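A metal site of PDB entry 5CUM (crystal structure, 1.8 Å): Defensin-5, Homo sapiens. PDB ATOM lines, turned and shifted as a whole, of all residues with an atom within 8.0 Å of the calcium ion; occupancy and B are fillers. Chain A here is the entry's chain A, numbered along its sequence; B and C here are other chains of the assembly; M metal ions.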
ATOM      1  N   CYS A  20       0.113 -28.069  24.474  1.00  0.00           N
ATOM      2  CA  CYS A  20      -0.718 -28.627  23.413  1.00  0.00           C
ATOM      3  C   CYS A  20      -2.176 -28.513  23.860  1.00  0.00           C
ATOM      4  O   CYS A  20      -2.486 -27.844  24.861  1.00  0.00           O
ATOM      5  CB  CYS A  20      -0.320 -30.072  23.126  1.00  0.00           C
ATOM      6  SG  CYS A  20      -0.356 -31.112  24.634  1.00  0.00           S
ATOM      7  N   GLU A  21      -3.060 -29.124  23.089  1.00  0.00           N
ATOM      8  CA  GLU A  21      -4.485 -29.069  23.420  1.00  0.00           C
ATOM      9  C   GLU A  21      -5.130 -30.425  23.268  1.00  0.00           C
ATOM     10  O   GLU A  21      -4.801 -31.197  22.376  1.00  0.00           O
ATOM     11  CB  GLU A  21      -5.213 -28.055  22.535  1.00  0.00           C
ATOM     12  CG  GLU A  21      -5.082 -26.623  23.018  1.00  0.00           C
ATOM     13  CD  GLU A  21      -5.949 -25.694  22.188  1.00  0.00           C
ATOM     14  OE1 GLU A  21      -6.006 -25.907  20.958  1.00  0.00           O
ATOM     15  OE2 GLU A  21      -6.566 -24.745  22.778  1.00  0.00           O
ATOM     16  N   ILE A  22      -6.074 -30.703  24.147  1.00  0.00           N
ATOM     17  CA  ILE A  22      -6.908 -31.878  23.988  1.00  0.00           C
ATOM     18  C   ILE A  22      -8.323 -31.377  23.880  1.00  0.00           C
ATOM     19  O   ILE A  22      -8.828 -30.772  24.824  1.00  0.00           O
ATOM     20  CB  ILE A  22      -6.740 -32.841  25.165  1.00  0.00           C
ATOM     21  CG1 ILE A  22      -5.283 -33.319  25.247  1.00  0.00           C
ATOM     22  CG2 ILE A  22      -7.702 -34.019  25.006  1.00  0.00           C
ATOM     23  CD1 ILE A  22      -4.940 -34.084  26.493  1.00  0.00           C
ATOM     24  N   SER A  23      -8.927 -31.594  22.726  1.00  0.00           N
ATOM     25  CA  SER A  23     -10.269 -31.085  22.446  1.00  0.00           C
ATOM     26  C   SER A  23     -10.357 -29.601  22.760  1.00  0.00           C
ATOM     27  O   SER A  23     -11.326 -29.149  23.358  1.00  0.00           O
ATOM     28  CB  SER A  23     -11.314 -31.867  23.228  1.00  0.00           C
ATOM     29  OG  SER A  23     -11.377 -33.189  22.732  1.00  0.00           O
ATOM     30  N   GLY A  24      -9.326 -28.851  22.389  1.00  0.00           N
ATOM     31  CA  GLY A  24      -9.397 -27.403  22.463  1.00  0.00           C
ATOM     32  C   GLY A  24      -9.124 -26.829  23.834  1.00  0.00           C
ATOM     33  O   GLY A  24      -9.338 -25.636  24.047  1.00  0.00           O
ATOM     34  N   ARG A  25      -8.695 -27.679  24.771  1.00  0.00           N
ATOM     35  CA  ARG A  25      -8.326 -27.222  26.105  1.00  0.00           C
ATOM     36  C   ARG A  25      -6.853 -27.454  26.312  1.00  0.00           C
ATOM     37  O   ARG A  25      -6.344 -28.522  25.980  1.00  0.00           O
ATOM     38  CB  ARG A  25      -9.126 -27.947  27.198  1.00  0.00           C
ATOM     39  CG  ARG A  25     -10.630 -27.903  26.957  1.00  0.00           C
ATOM     40  CD  ARG A  25     -11.398 -27.793  28.234  1.00  0.00           C
ATOM     41  NE  ARG A  25     -12.760 -27.319  27.966  1.00  0.00           N
ATOM     42  CZ  ARG A  25     -13.560 -26.794  28.885  1.00  0.00           C
ATOM     43  NH1 ARG A  25     -13.153 -26.662  30.132  1.00  0.00           N
ATOM     44  NH2 ARG A  25     -14.785 -26.403  28.541  1.00  0.00           N
ATOM     45  N   LEU A  26      -6.179 -26.432  26.838  1.00  0.00           N
ATOM     46  CA  LEU A  26      -4.745 -26.487  27.064  1.00  0.00           C
ATOM     47  C   LEU A  26      -4.382 -27.692  27.906  1.00  0.00           C
ATOM     48  O   LEU A  26      -5.110 -28.050  28.853  1.00  0.00           O
ATOM     49  CB  LEU A  26      -4.237 -25.204  27.762  1.00  0.00           C
ATOM     50  CG  LEU A  26      -4.431 -23.885  27.023  1.00  0.00           C
ATOM     51  CD1 LEU A  26      -3.902 -22.716  27.842  1.00  0.00           C
ATOM     52  CD2 LEU A  26      -3.806 -23.900  25.619  1.00  0.00           C
ATOM     53  N   CYS B  20      -4.988 -18.150  30.706  1.00  0.00           N
ATOM     54  CA  CYS B  20      -5.833 -19.233  31.155  1.00  0.00           C
ATOM     55  C   CYS B  20      -6.917 -19.419  30.097  1.00  0.00           C
ATOM     56  O   CYS B  20      -6.842 -18.839  29.000  1.00  0.00           O
ATOM     57  CB  CYS B  20      -6.434 -18.919  32.529  1.00  0.00           C
ATOM     58  SG  CYS B  20      -7.291 -17.278  32.530  1.00  0.00           S
ATOM     59  N   GLU B  21      -7.899 -20.265  30.394  1.00  0.00           N
ATOM     60  CA  GLU B  21      -8.966 -20.499  29.423  1.00  0.00           C
ATOM     61  C   GLU B  21     -10.305 -20.484  30.096  1.00  0.00           C
ATOM     62  O   GLU B  21     -10.451 -20.948  31.227  1.00  0.00           O
ATOM     63  CB  GLU B  21      -8.785 -21.843  28.718  1.00  0.00           C
ATOM     64  CG  GLU B  21      -7.795 -21.817  27.594  1.00  0.00           C
ATOM     65  CD  GLU B  21      -7.790 -23.144  26.853  1.00  0.00           C
ATOM     66  OE1 GLU B  21      -7.797 -24.189  27.543  1.00  0.00           O
ATOM     67  OE2 GLU B  21      -7.801 -23.160  25.587  1.00  0.00           O
ATOM     68  N   ILE B  22     -11.305 -19.973  29.387  1.00  0.00           N
ATOM     69  CA  ILE B  22     -12.673 -20.091  29.859  1.00  0.00           C
ATOM     70  C   ILE B  22     -13.408 -20.854  28.776  1.00  0.00           C
ATOM     71  O   ILE B  22     -13.458 -20.394  27.640  1.00  0.00           O
ATOM     72  CB  ILE B  22     -13.324 -18.726  30.099  1.00  0.00           C
ATOM     73  CG1 ILE B  22     -12.527 -17.929  31.149  1.00  0.00           C
ATOM     74  CG2 ILE B  22     -14.785 -18.905  30.487  1.00  0.00           C
ATOM     75  CD1 ILE B  22     -12.916 -16.477  31.280  1.00  0.00           C
ATOM     76  N   SER B  23     -13.957 -22.011  29.134  1.00  0.00           N
ATOM     77  CA  SER B  23     -14.579 -22.909  28.178  1.00  0.00           C
ATOM     78  C   SER B  23     -13.711 -23.143  26.949  1.00  0.00           C
ATOM     79  O   SER B  23     -14.202 -23.168  25.828  1.00  0.00           O
ATOM     80  CB  SER B  23     -15.948 -22.363  27.759  1.00  0.00           C
ATOM     81  OG  SER B  23     -16.778 -22.289  28.892  1.00  0.00           O
ATOM     82  N   GLY B  24     -12.400 -23.273  27.160  1.00  0.00           N
ATOM     83  CA  GLY B  24     -11.524 -23.679  26.080  1.00  0.00           C
ATOM     84  C   GLY B  24     -11.078 -22.518  25.205  1.00  0.00           C
ATOM     85  O   GLY B  24     -10.454 -22.742  24.165  1.00  0.00           O
ATOM     86  N   ARG B  25     -11.427 -21.302  25.610  1.00  0.00           N
ATOM     87  CA  ARG B  25     -10.974 -20.123  24.879  1.00  0.00           C
ATOM     88  C   ARG B  25     -10.012 -19.322  25.717  1.00  0.00           C
ATOM     89  O   ARG B  25     -10.272 -19.078  26.905  1.00  0.00           O
ATOM     90  CB  ARG B  25     -12.152 -19.234  24.473  1.00  0.00           C
ATOM     91  CG  ARG B  25     -13.092 -19.964  23.533  1.00  0.00           C
ATOM     92  CD  ARG B  25     -14.336 -19.158  23.242  1.00  0.00           C
ATOM     93  NE  ARG B  25     -14.912 -19.412  21.913  1.00  0.00           N
ATOM     94  CZ  ARG B  25     -15.072 -20.604  21.305  1.00  0.00           C
ATOM     95  NH1 ARG B  25     -14.750 -21.750  21.906  1.00  0.00           N
ATOM     96  NH2 ARG B  25     -15.605 -20.637  20.091  1.00  0.00           N
ATOM     97  N   LEU B  26      -8.912 -18.903  25.091  1.00  0.00           N
ATOM     98  CA  LEU B  26      -7.883 -18.123  25.771  1.00  0.00           C
ATOM     99  C   LEU B  26      -8.488 -16.896  26.436  1.00  0.00           C
ATOM    100  O   LEU B  26      -9.401 -16.248  25.900  1.00  0.00           O
ATOM    101  CB  LEU B  26      -6.790 -17.681  24.782  1.00  0.00           C
ATOM    102  CG  LEU B  26      -6.010 -18.807  24.078  1.00  0.00           C
ATOM    103  CD1 LEU B  26      -4.904 -18.253  23.176  1.00  0.00           C
ATOM    104  CD2 LEU B  26      -5.456 -19.850  25.062  1.00  0.00           C
ATOM    105  N   CYS C  20      -3.122 -17.475  18.052  1.00  0.00           N
ATOM    106  CA  CYS C  20      -4.524 -17.089  18.158  1.00  0.00           C
ATOM    107  C   CYS C  20      -5.345 -18.388  18.235  1.00  0.00           C
ATOM    108  O   CYS C  20      -4.772 -19.486  18.396  1.00  0.00           O
ATOM    109  CB  CYS C  20      -4.937 -16.207  16.978  1.00  0.00           C
ATOM    110  SG  CYS C  20      -4.497 -17.004  15.373  1.00  0.00           S
ATOM    111  N   GLU C  21      -6.651 -18.262  18.173  1.00  0.00           N
ATOM    112  CA  GLU C  21      -7.516 -19.441  18.206  1.00  0.00           C
ATOM    113  C   GLU C  21      -8.602 -19.358  17.149  1.00  0.00           C
ATOM    114  O   GLU C  21      -9.126 -18.292  16.869  1.00  0.00           O
ATOM    115  CB  GLU C  21      -8.174 -19.604  19.562  1.00  0.00           C
ATOM    116  CG  GLU C  21      -7.268 -20.168  20.614  1.00  0.00           C
ATOM    117  CD  GLU C  21      -8.030 -20.452  21.905  1.00  0.00           C
ATOM    118  OE1 GLU C  21      -8.778 -19.572  22.340  1.00  0.00           O
ATOM    119  OE2 GLU C  21      -7.845 -21.552  22.495  1.00  0.00           O
ATOM    120  N   ILE C  22      -8.939 -20.504  16.582  1.00  0.00           N
ATOM    121  CA  ILE C  22     -10.105 -20.547  15.728  1.00  0.00           C
ATOM    122  C   ILE C  22     -11.066 -21.514  16.378  1.00  0.00           C
ATOM    123  O   ILE C  22     -10.725 -22.675  16.556  1.00  0.00           O
ATOM    124  CB  ILE C  22      -9.746 -21.012  14.313  1.00  0.00           C
ATOM    125  CG1 ILE C  22      -8.763 -20.009  13.683  1.00  0.00           C
ATOM    126  CG2 ILE C  22     -11.020 -21.210  13.494  1.00  0.00           C
ATOM    127  CD1 ILE C  22      -8.140 -20.462  12.393  1.00  0.00           C
ATOM    128  N   SER C  23     -12.226 -21.014  16.783  1.00  0.00           N
ATOM    129  CA  SER C  23     -13.186 -21.807  17.536  1.00  0.00           C
ATOM    130  C   SER C  23     -12.524 -22.544  18.697  1.00  0.00           C
ATOM    131  O   SER C  23     -12.756 -23.723  18.906  1.00  0.00           O
ATOM    132  CB  SER C  23     -13.894 -22.795  16.608  1.00  0.00           C
ATOM    133  OG  SER C  23     -14.710 -22.086  15.696  1.00  0.00           O
ATOM    134  N   GLY C  24     -11.661 -21.836  19.424  1.00  0.00           N
ATOM    135  CA  GLY C  24     -11.109 -22.393  20.649  1.00  0.00           C
ATOM    136  C   GLY C  24      -9.958 -23.365  20.468  1.00  0.00           C
ATOM    137  O   GLY C  24      -9.531 -24.000  21.437  1.00  0.00           O
ATOM    138  N   ARG C  25      -9.489 -23.513  19.239  1.00  0.00           N
ATOM    139  CA  ARG C  25      -8.323 -24.329  18.990  1.00  0.00           C
ATOM    140  C   ARG C  25      -7.183 -23.460  18.529  1.00  0.00           C
ATOM    141  O   ARG C  25      -7.379 -22.573  17.673  1.00  0.00           O
ATOM    142  CB  ARG C  25      -8.596 -25.429  17.949  1.00  0.00           C
ATOM    143  CG  ARG C  25      -9.851 -26.229  18.264  1.00  0.00           C
ATOM    144  CD  ARG C  25      -9.641 -27.709  18.074  1.00  0.00           C
ATOM    145  NE  ARG C  25     -10.761 -28.470  18.624  1.00  0.00           N
ATOM    146  CZ  ARG C  25     -10.795 -29.798  18.722  1.00  0.00           C
ATOM    147  NH1 ARG C  25      -9.762 -30.526  18.307  1.00  0.00           N
ATOM    148  NH2 ARG C  25     -11.862 -30.388  19.221  1.00  0.00           N
ATOM    149  N   LEU C  26      -6.009 -23.698  19.103  1.00  0.00           N
ATOM    150  CA  LEU C  26      -4.815 -22.923  18.798  1.00  0.00           C
ATOM    151  C   LEU C  26      -4.537 -22.907  17.303  1.00  0.00           C
ATOM    152  O   LEU C  26      -4.750 -23.922  16.617  1.00  0.00           O
ATOM    153  CB  LEU C  26      -3.586 -23.502  19.524  1.00  0.00           C
ATOM    154  CG  LEU C  26      -3.679 -23.518  21.054  1.00  0.00           C
ATOM    155  CD1 LEU C  26      -2.412 -24.089  21.673  1.00  0.00           C
ATOM    156  CD2 LEU C  26      -4.004 -22.134  21.622  1.00  0.00           C
HETATM  157 CA    CA M   1      -8.412 -23.565  23.430  1.00  0.00          CA
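The side-chain carboxylate (OE1) of Glu 21 of chain B sits at hydrogen-bond distance from the backbone NH (N) of Leu 26 of chain A, at 2.9 Å. The side-chain carboxylate of Glu 21 of chain C sits at hydrogen-bond distance from the backbone NH of Leu 26 of chain B (2.8 Å). The side-chain carboxylate of Glu 21 of chain A lies within hydrogen-bond range of the backbone NH of Leu 26 of chain C (2.9 Å).
Within 4 Å of the calcium ion: Glu 21 of chain A, Gly 24 of chain A, Glu 21 of chain B, Gly 24 of chain B, Glu 21 of chain C and Gly 24 of chain C. The nearest printed residue that does not touch the calcium ion is Arg 25 of chain C (4.3 Å).
The calcium ion is bound by OE2 of Glu 21 of chain B (2.3 Å), OE2 of Glu 21 of chain A (2.3 Å), OE2 of Glu 21 of chain C (2.3 Å), O of Gly 24 of chain B (2.3 Å), O of Gly 24 of chain C (2.3 Å) and O of Gly 24 of chain A (2.4 Å). The calcium ion has six donor atoms within binding distance.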
